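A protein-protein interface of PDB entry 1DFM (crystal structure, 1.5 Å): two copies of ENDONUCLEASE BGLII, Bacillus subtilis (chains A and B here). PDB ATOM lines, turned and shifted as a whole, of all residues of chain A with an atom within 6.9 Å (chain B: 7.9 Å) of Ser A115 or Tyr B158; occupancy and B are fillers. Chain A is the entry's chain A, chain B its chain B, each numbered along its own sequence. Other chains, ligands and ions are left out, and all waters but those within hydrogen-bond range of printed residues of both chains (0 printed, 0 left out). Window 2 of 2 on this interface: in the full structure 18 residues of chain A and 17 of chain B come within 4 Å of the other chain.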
ATOM      1  N   PHE A  76     -32.344   4.907  13.328  1.00  0.00           N
ATOM      2  CA  PHE A  76     -31.511   4.745  14.508  1.00  0.00           C
ATOM      3  C   PHE A  76     -31.227   3.256  14.709  1.00  0.00           C
ATOM      4  O   PHE A  76     -30.864   2.852  15.800  1.00  0.00           O
ATOM      5  CB  PHE A  76     -32.194   5.321  15.758  1.00  0.00           C
ATOM      6  CG  PHE A  76     -31.943   6.806  15.983  1.00  0.00           C
ATOM      7  CD1 PHE A  76     -30.692   7.373  15.733  1.00  0.00           C
ATOM      8  CD2 PHE A  76     -32.947   7.619  16.491  1.00  0.00           C
ATOM      9  CE1 PHE A  76     -30.435   8.730  15.981  1.00  0.00           C
ATOM     10  CE2 PHE A  76     -32.713   8.999  16.753  1.00  0.00           C
ATOM     11  CZ  PHE A  76     -31.454   9.557  16.496  1.00  0.00           C
ATOM     12  N   GLU A 110     -30.593   9.562  24.954  1.00  0.00           N
ATOM     13  CA  GLU A 110     -30.301  10.965  24.677  1.00  0.00           C
ATOM     14  C   GLU A 110     -30.532  11.218  23.198  1.00  0.00           C
ATOM     15  O   GLU A 110     -31.156  12.221  22.837  1.00  0.00           O
ATOM     16  CB  GLU A 110     -28.842  11.303  25.048  1.00  0.00           C
ATOM     17  CG  GLU A 110     -28.371  12.707  24.591  1.00  0.00           C
ATOM     18  CD  GLU A 110     -29.066  13.824  25.345  1.00  0.00           C
ATOM     19  OE1 GLU A 110     -30.044  13.552  26.075  1.00  0.00           O
ATOM     20  OE2 GLU A 110     -28.635  14.995  25.192  1.00  0.00           O
ATOM     21  N   LEU A 111     -30.038  10.339  22.343  1.00  0.00           N
ATOM     22  CA  LEU A 111     -30.207  10.540  20.905  1.00  0.00           C
ATOM     23  C   LEU A 111     -31.694  10.432  20.523  1.00  0.00           C
ATOM     24  O   LEU A 111     -32.182  11.220  19.709  1.00  0.00           O
ATOM     25  CB  LEU A 111     -29.371   9.548  20.105  1.00  0.00           C
ATOM     26  CG  LEU A 111     -27.865   9.794  20.257  1.00  0.00           C
ATOM     27  CD1 LEU A 111     -27.031   8.649  19.664  1.00  0.00           C
ATOM     28  CD2 LEU A 111     -27.541  11.122  19.584  1.00  0.00           C
ATOM     29  N   PHE A 112     -32.417   9.463  21.070  1.00  0.00           N
ATOM     30  CA  PHE A 112     -33.853   9.405  20.736  1.00  0.00           C
ATOM     31  C   PHE A 112     -34.517  10.741  21.107  1.00  0.00           C
ATOM     32  O   PHE A 112     -35.346  11.288  20.347  1.00  0.00           O
ATOM     33  CB  PHE A 112     -34.552   8.284  21.514  1.00  0.00           C
ATOM     34  CG  PHE A 112     -33.973   6.921  21.306  1.00  0.00           C
ATOM     35  CD1 PHE A 112     -33.267   6.598  20.158  1.00  0.00           C
ATOM     36  CD2 PHE A 112     -34.180   5.939  22.269  1.00  0.00           C
ATOM     37  CE1 PHE A 112     -32.766   5.299  19.975  1.00  0.00           C
ATOM     38  CE2 PHE A 112     -33.692   4.649  22.083  1.00  0.00           C
ATOM     39  CZ  PHE A 112     -32.990   4.347  20.941  1.00  0.00           C
ATOM     40  N   HIS A 113     -34.200  11.261  22.279  1.00  0.00           N
ATOM     41  CA  HIS A 113     -34.788  12.524  22.728  1.00  0.00           C
ATOM     42  C   HIS A 113     -34.433  13.704  21.824  1.00  0.00           C
ATOM     43  O   HIS A 113     -35.291  14.528  21.524  1.00  0.00           O
ATOM     44  CB  HIS A 113     -34.354  12.827  24.157  1.00  0.00           C
ATOM     45  CG  HIS A 113     -35.024  14.025  24.765  1.00  0.00           C
ATOM     46  ND1 HIS A 113     -34.422  15.264  24.824  1.00  0.00           N
ATOM     47  CD2 HIS A 113     -36.207  14.156  25.415  1.00  0.00           C
ATOM     48  CE1 HIS A 113     -35.199  16.105  25.493  1.00  0.00           C
ATOM     49  NE2 HIS A 113     -36.289  15.457  25.861  1.00  0.00           N
ATOM     50  N   LYS A 114     -33.180  13.793  21.392  1.00  0.00           N
ATOM     51  CA  LYS A 114     -32.778  14.915  20.533  1.00  0.00           C
ATOM     52  C   LYS A 114     -33.509  14.952  19.223  1.00  0.00           C
ATOM     53  O   LYS A 114     -33.837  16.033  18.716  1.00  0.00           O
ATOM     54  CB  LYS A 114     -31.290  14.863  20.234  1.00  0.00           C
ATOM     55  CG  LYS A 114     -30.481  15.365  21.368  1.00  0.00           C
ATOM     56  CD  LYS A 114     -29.069  15.658  20.917  1.00  0.00           C
ATOM     57  CE  LYS A 114     -28.238  16.116  22.079  1.00  0.00           C
ATOM     58  NZ  LYS A 114     -28.445  17.544  22.476  1.00  0.00           N
ATOM     59  N   SER A 115     -33.752  13.775  18.668  1.00  0.00           N
ATOM     60  CA  SER A 115     -34.444  13.639  17.395  1.00  0.00           C
ATOM     61  C   SER A 115     -35.953  13.605  17.562  1.00  0.00           C
ATOM     62  O   SER A 115     -36.694  13.691  16.582  1.00  0.00           O
ATOM     63  CB  SER A 115     -34.002  12.358  16.710  1.00  0.00           C
ATOM     64  OG  SER A 115     -34.209  11.256  17.564  1.00  0.00           O
ATOM     65  N   ASN A 116     -36.406  13.491  18.802  1.00  0.00           N
ATOM     66  CA  ASN A 116     -37.828  13.432  19.132  1.00  0.00           C
ATOM     67  C   ASN A 116     -38.542  12.145  18.716  1.00  0.00           C
ATOM     68  O   ASN A 116     -39.648  12.155  18.162  1.00  0.00           O
ATOM     69  CB  ASN A 116     -38.595  14.627  18.550  1.00  0.00           C
ATOM     70  CG  ASN A 116     -39.976  14.767  19.163  1.00  0.00           C
ATOM     71  OD1 ASN A 116     -40.109  14.950  20.394  1.00  0.00           O
ATOM     72  ND2 ASN A 116     -41.016  14.674  18.331  1.00  0.00           N
ATOM     73  N   MET A 117     -37.897  11.018  18.998  1.00  0.00           N
ATOM     74  CA  MET A 117     -38.458   9.703  18.702  1.00  0.00           C
ATOM     75  C   MET A 117     -39.856   9.454  19.270  1.00  0.00           C
ATOM     76  O   MET A 117     -40.128   9.729  20.444  1.00  0.00           O
ATOM     77  CB  MET A 117     -37.538   8.588  19.251  1.00  0.00           C
ATOM     78  CG  MET A 117     -38.287   7.293  19.575  1.00  0.00           C
ATOM     79  SD  MET A 117     -37.136   5.926  19.935  1.00  0.00           S
ATOM     80  CE  MET A 117     -36.045   6.109  18.391  1.00  0.00           C
ATOM     81  N   ASP A 118     -40.742   8.931  18.429  1.00  0.00           N
ATOM     82  CA  ASP A 118     -42.087   8.597  18.903  1.00  0.00           C
ATOM     83  C   ASP A 118     -41.881   7.401  19.806  1.00  0.00           C
ATOM     84  O   ASP A 118     -41.038   6.564  19.520  1.00  0.00           O
ATOM     85  CB  ASP A 118     -42.994   8.136  17.760  1.00  0.00           C
ATOM     86  CG  ASP A 118     -43.210   9.202  16.735  1.00  0.00           C
ATOM     87  OD1 ASP A 118     -44.031  10.113  16.998  1.00  0.00           O
ATOM     88  OD2 ASP A 118     -42.545   9.139  15.673  1.00  0.00           O
ATOM     89  N   GLN B 151     -22.364   4.313  15.495  1.00  0.00           N
ATOM     90  CA  GLN B 151     -22.735   4.952  16.762  1.00  0.00           C
ATOM     91  C   GLN B 151     -21.988   6.245  16.993  1.00  0.00           C
ATOM     92  O   GLN B 151     -22.613   7.266  17.317  1.00  0.00           O
ATOM     93  CB  GLN B 151     -22.528   3.995  17.933  1.00  0.00           C
ATOM     94  CG  GLN B 151     -23.487   2.812  17.874  1.00  0.00           C
ATOM     95  CD  GLN B 151     -23.546   2.000  19.152  1.00  0.00           C
ATOM     96  OE1 GLN B 151     -22.708   2.154  20.044  1.00  0.00           O
ATOM     97  NE2 GLN B 151     -24.532   1.110  19.239  1.00  0.00           N
ATOM     98  N   LEU B 152     -20.669   6.247  16.821  1.00  0.00           N
ATOM     99  CA  LEU B 152     -19.933   7.492  17.055  1.00  0.00           C
ATOM    100  C   LEU B 152     -20.276   8.547  15.997  1.00  0.00           C
ATOM    101  O   LEU B 152     -20.255   9.762  16.318  1.00  0.00           O
ATOM    102  CB  LEU B 152     -18.420   7.226  17.059  1.00  0.00           C
ATOM    103  CG  LEU B 152     -17.953   6.362  18.248  1.00  0.00           C
ATOM    104  CD1 LEU B 152     -16.425   6.168  18.163  1.00  0.00           C
ATOM    105  CD2 LEU B 152     -18.373   7.044  19.554  1.00  0.00           C
ATOM    106  N   ASN B 153     -20.576   8.124  14.763  1.00  0.00           N
ATOM    107  CA  ASN B 153     -20.972   9.084  13.709  1.00  0.00           C
ATOM    108  C   ASN B 153     -22.249   9.782  14.129  1.00  0.00           C
ATOM    109  O   ASN B 153     -22.401  10.989  13.912  1.00  0.00           O
ATOM    110  CB  ASN B 153     -21.262   8.364  12.351  1.00  0.00           C
ATOM    111  CG  ASN B 153     -20.006   7.968  11.568  1.00  0.00           C
ATOM    112  OD1 ASN B 153     -20.105   7.287  10.516  1.00  0.00           O
ATOM    113  ND2 ASN B 153     -18.849   8.364  12.032  1.00  0.00           N
ATOM    114  N   SER B 154     -23.187   9.045  14.708  1.00  0.00           N
ATOM    115  CA  SER B 154     -24.437   9.654  15.126  1.00  0.00           C
ATOM    116  C   SER B 154     -24.189  10.596  16.302  1.00  0.00           C
ATOM    117  O   SER B 154     -24.711  11.732  16.311  1.00  0.00           O
ATOM    118  CB  SER B 154     -25.417   8.557  15.471  1.00  0.00           C
ATOM    119  OG  SER B 154     -26.684   9.082  15.816  1.00  0.00           O
ATOM    120  N   LEU B 155     -23.373  10.185  17.264  1.00  0.00           N
ATOM    121  CA  LEU B 155     -23.039  11.082  18.383  1.00  0.00           C
ATOM    122  C   LEU B 155     -22.377  12.354  17.847  1.00  0.00           C
ATOM    123  O   LEU B 155     -22.665  13.455  18.348  1.00  0.00           O
ATOM    124  CB  LEU B 155     -22.072  10.427  19.367  1.00  0.00           C
ATOM    125  CG  LEU B 155     -22.763   9.578  20.422  1.00  0.00           C
ATOM    126  CD1 LEU B 155     -23.519   8.453  19.794  1.00  0.00           C
ATOM    127  CD2 LEU B 155     -21.681   9.035  21.380  1.00  0.00           C
ATOM    128  N   ALA B 156     -21.530  12.223  16.817  1.00  0.00           N
ATOM    129  CA  ALA B 156     -20.860  13.409  16.264  1.00  0.00           C
ATOM    130  C   ALA B 156     -21.853  14.307  15.528  1.00  0.00           C
ATOM    131  O   ALA B 156     -21.791  15.531  15.636  1.00  0.00           O
ATOM    132  CB  ALA B 156     -19.714  12.976  15.346  1.00  0.00           C
ATOM    133  N   GLU B 157     -22.816  13.709  14.826  1.00  0.00           N
ATOM    134  CA  GLU B 157     -23.816  14.520  14.124  1.00  0.00           C
ATOM    135  C   GLU B 157     -24.599  15.364  15.129  1.00  0.00           C
ATOM    136  O   GLU B 157     -25.020  16.470  14.820  1.00  0.00           O
ATOM    137  CB  GLU B 157     -24.766  13.609  13.355  1.00  0.00           C
ATOM    138  CG  GLU B 157     -25.994  14.294  12.719  1.00  0.00           C
ATOM    139  CD  GLU B 157     -27.034  13.297  12.171  1.00  0.00           C
ATOM    140  OE1 GLU B 157     -26.822  12.064  12.258  1.00  0.00           O
ATOM    141  OE2 GLU B 157     -28.090  13.771  11.670  1.00  0.00           O
ATOM    142  N   TYR B 158     -24.773  14.854  16.348  1.00  0.00           N
ATOM    143  CA  TYR B 158     -25.516  15.607  17.352  1.00  0.00           C
ATOM    144  C   TYR B 158     -24.604  16.320  18.363  1.00  0.00           C
ATOM    145  O   TYR B 158     -25.067  16.779  19.399  1.00  0.00           O
ATOM    146  CB  TYR B 158     -26.510  14.667  18.067  1.00  0.00           C
ATOM    147  CG  TYR B 158     -27.704  14.273  17.212  1.00  0.00           C
ATOM    148  CD1 TYR B 158     -28.837  15.071  17.180  1.00  0.00           C
ATOM    149  CD2 TYR B 158     -27.700  13.108  16.458  1.00  0.00           C
ATOM    150  CE1 TYR B 158     -29.954  14.721  16.424  1.00  0.00           C
ATOM    151  CE2 TYR B 158     -28.796  12.748  15.696  1.00  0.00           C
ATOM    152  CZ  TYR B 158     -29.923  13.557  15.688  1.00  0.00           C
ATOM    153  OH  TYR B 158     -31.030  13.200  14.931  1.00  0.00           O
ATOM    154  N   ASN B 159     -23.311  16.416  18.039  1.00  0.00           N
ATOM    155  CA  ASN B 159     -22.322  17.119  18.866  1.00  0.00           C
ATOM    156  C   ASN B 159     -22.387  16.685  20.336  1.00  0.00           C
ATOM    157  O   ASN B 159     -22.274  17.524  21.252  1.00  0.00           O
ATOM    158  CB  ASN B 159     -22.573  18.631  18.711  1.00  0.00           C
ATOM    159  CG  ASN B 159     -21.391  19.513  19.138  1.00  0.00           C
ATOM    160  OD1 ASN B 159     -21.607  20.681  19.583  1.00  0.00           O
ATOM    161  ND2 ASN B 159     -20.177  19.019  18.990  1.00  0.00           N
ATOM    162  N   VAL B 160     -22.473  15.374  20.580  1.00  0.00           N
ATOM    163  CA  VAL B 160     -22.575  14.876  21.937  1.00  0.00           C
ATOM    164  C   VAL B 160     -21.282  14.830  22.734  1.00  0.00           C
ATOM    165  O   VAL B 160     -21.280  15.092  23.948  1.00  0.00           O
ATOM    166  CB  VAL B 160     -23.217  13.452  21.958  1.00  0.00           C
ATOM    167  CG1 VAL B 160     -23.231  12.880  23.397  1.00  0.00           C
ATOM    168  CG2 VAL B 160     -24.657  13.511  21.383  1.00  0.00           C
ATOM    169  N   PHE B 161     -20.166  14.500  22.086  1.00  0.00           N
ATOM    170  CA  PHE B 161     -18.918  14.396  22.847  1.00  0.00           C
ATOM    171  C   PHE B 161     -17.841  15.249  22.195  1.00  0.00           C
ATOM    172  O   PHE B 161     -17.911  15.540  20.994  1.00  0.00           O
ATOM    173  CB  PHE B 161     -18.489  12.925  22.963  1.00  0.00           C
ATOM    174  CG  PHE B 161     -18.045  12.282  21.676  1.00  0.00           C
ATOM    175  CD1 PHE B 161     -18.951  11.738  20.791  1.00  0.00           C
ATOM    176  CD2 PHE B 161     -16.679  12.181  21.377  1.00  0.00           C
ATOM    177  CE1 PHE B 161     -18.517  11.101  19.614  1.00  0.00           C
ATOM    178  CE2 PHE B 161     -16.231  11.555  20.220  1.00  0.00           C
ATOM    179  CZ  PHE B 161     -17.145  11.015  19.327  1.00  0.00           C
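No position is printed for both chains. Of the 7 pairs that touch across the chains among the printed residues, none has its exchanged pair printed and touching as well.
Phe A76 touches Ser B154 (CE1 to OG, 3.8 Å). Phe A76 touches Tyr B158 (CZ to OH, 3.99 Å). OG of Ser B154 touches CD1 of Leu A111 (3.9 Å). Leu B155 touches Leu A111 (CD1 to CD1, 3.5 Å). CD2 of Leu A111 touches CD2 of Tyr B158 (3.7 Å). CD of Lys A114 touches CD1 of Tyr B158, at 3.8 Å. CB of Ser A115 touches OH of Tyr B158 (3.6 Å).
Printed residues of chain B within 4 Å of Phe A76: Ser B154 (3.8 Å) and Tyr B158 (3.99 Å). Of the printed residues of chain B, Leu A111 touches Ser B154 (3.9 Å), Leu B155 (3.5 Å) and Tyr B158 (3.7 Å). Of the printed residues of chain B, Lys A114 touches Tyr B158. Ser A115 touches just one residue of chain B: Tyr B158 (3.6 Å). Of the printed residues of chain A, Ser B154 touches Phe A76 and Leu A111. Printed residues of chain A within 4 Å of Leu B155: Leu A111 (3.5 Å). Of the printed residues of chain A, Tyr B158 touches Phe A76 (3.99 Å), Leu A111 (3.7 Å), Lys A114 (3.8 Å) and Ser A115 (3.6 Å). The nearest printed residue of chain B that does not touch Ser A115 is Glu B157 (7.9 Å).
O of Phe A112 lies within hydrogen-bond range of OG of Ser A115, 3.0 Å away. O of Leu A111 sits at hydrogen-bond distance from OG of Ser A115, at 3.0 Å. The side-chain carboxylate of Glu A110 lies within salt-bridge range of the side-chain amino group of Lys A114 (3.7 Å). The backbone NH of Val B160 is in hydrogen-bond range of the backbone carbonyl oxygen of Leu B155 (2.9 Å).
Hydrophobic or aromatic side chains of chain B that line the printed part of chain A: Leu B155 and Tyr B158. Hydrophobic or aromatic side chains of chain A that line the printed part of chain B: Phe A76 and Leu A111. Among the printed residues, no Asp or Glu carboxylate lies within 4 Å of a Lys or Arg side-chain nitrogen of the other chain.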
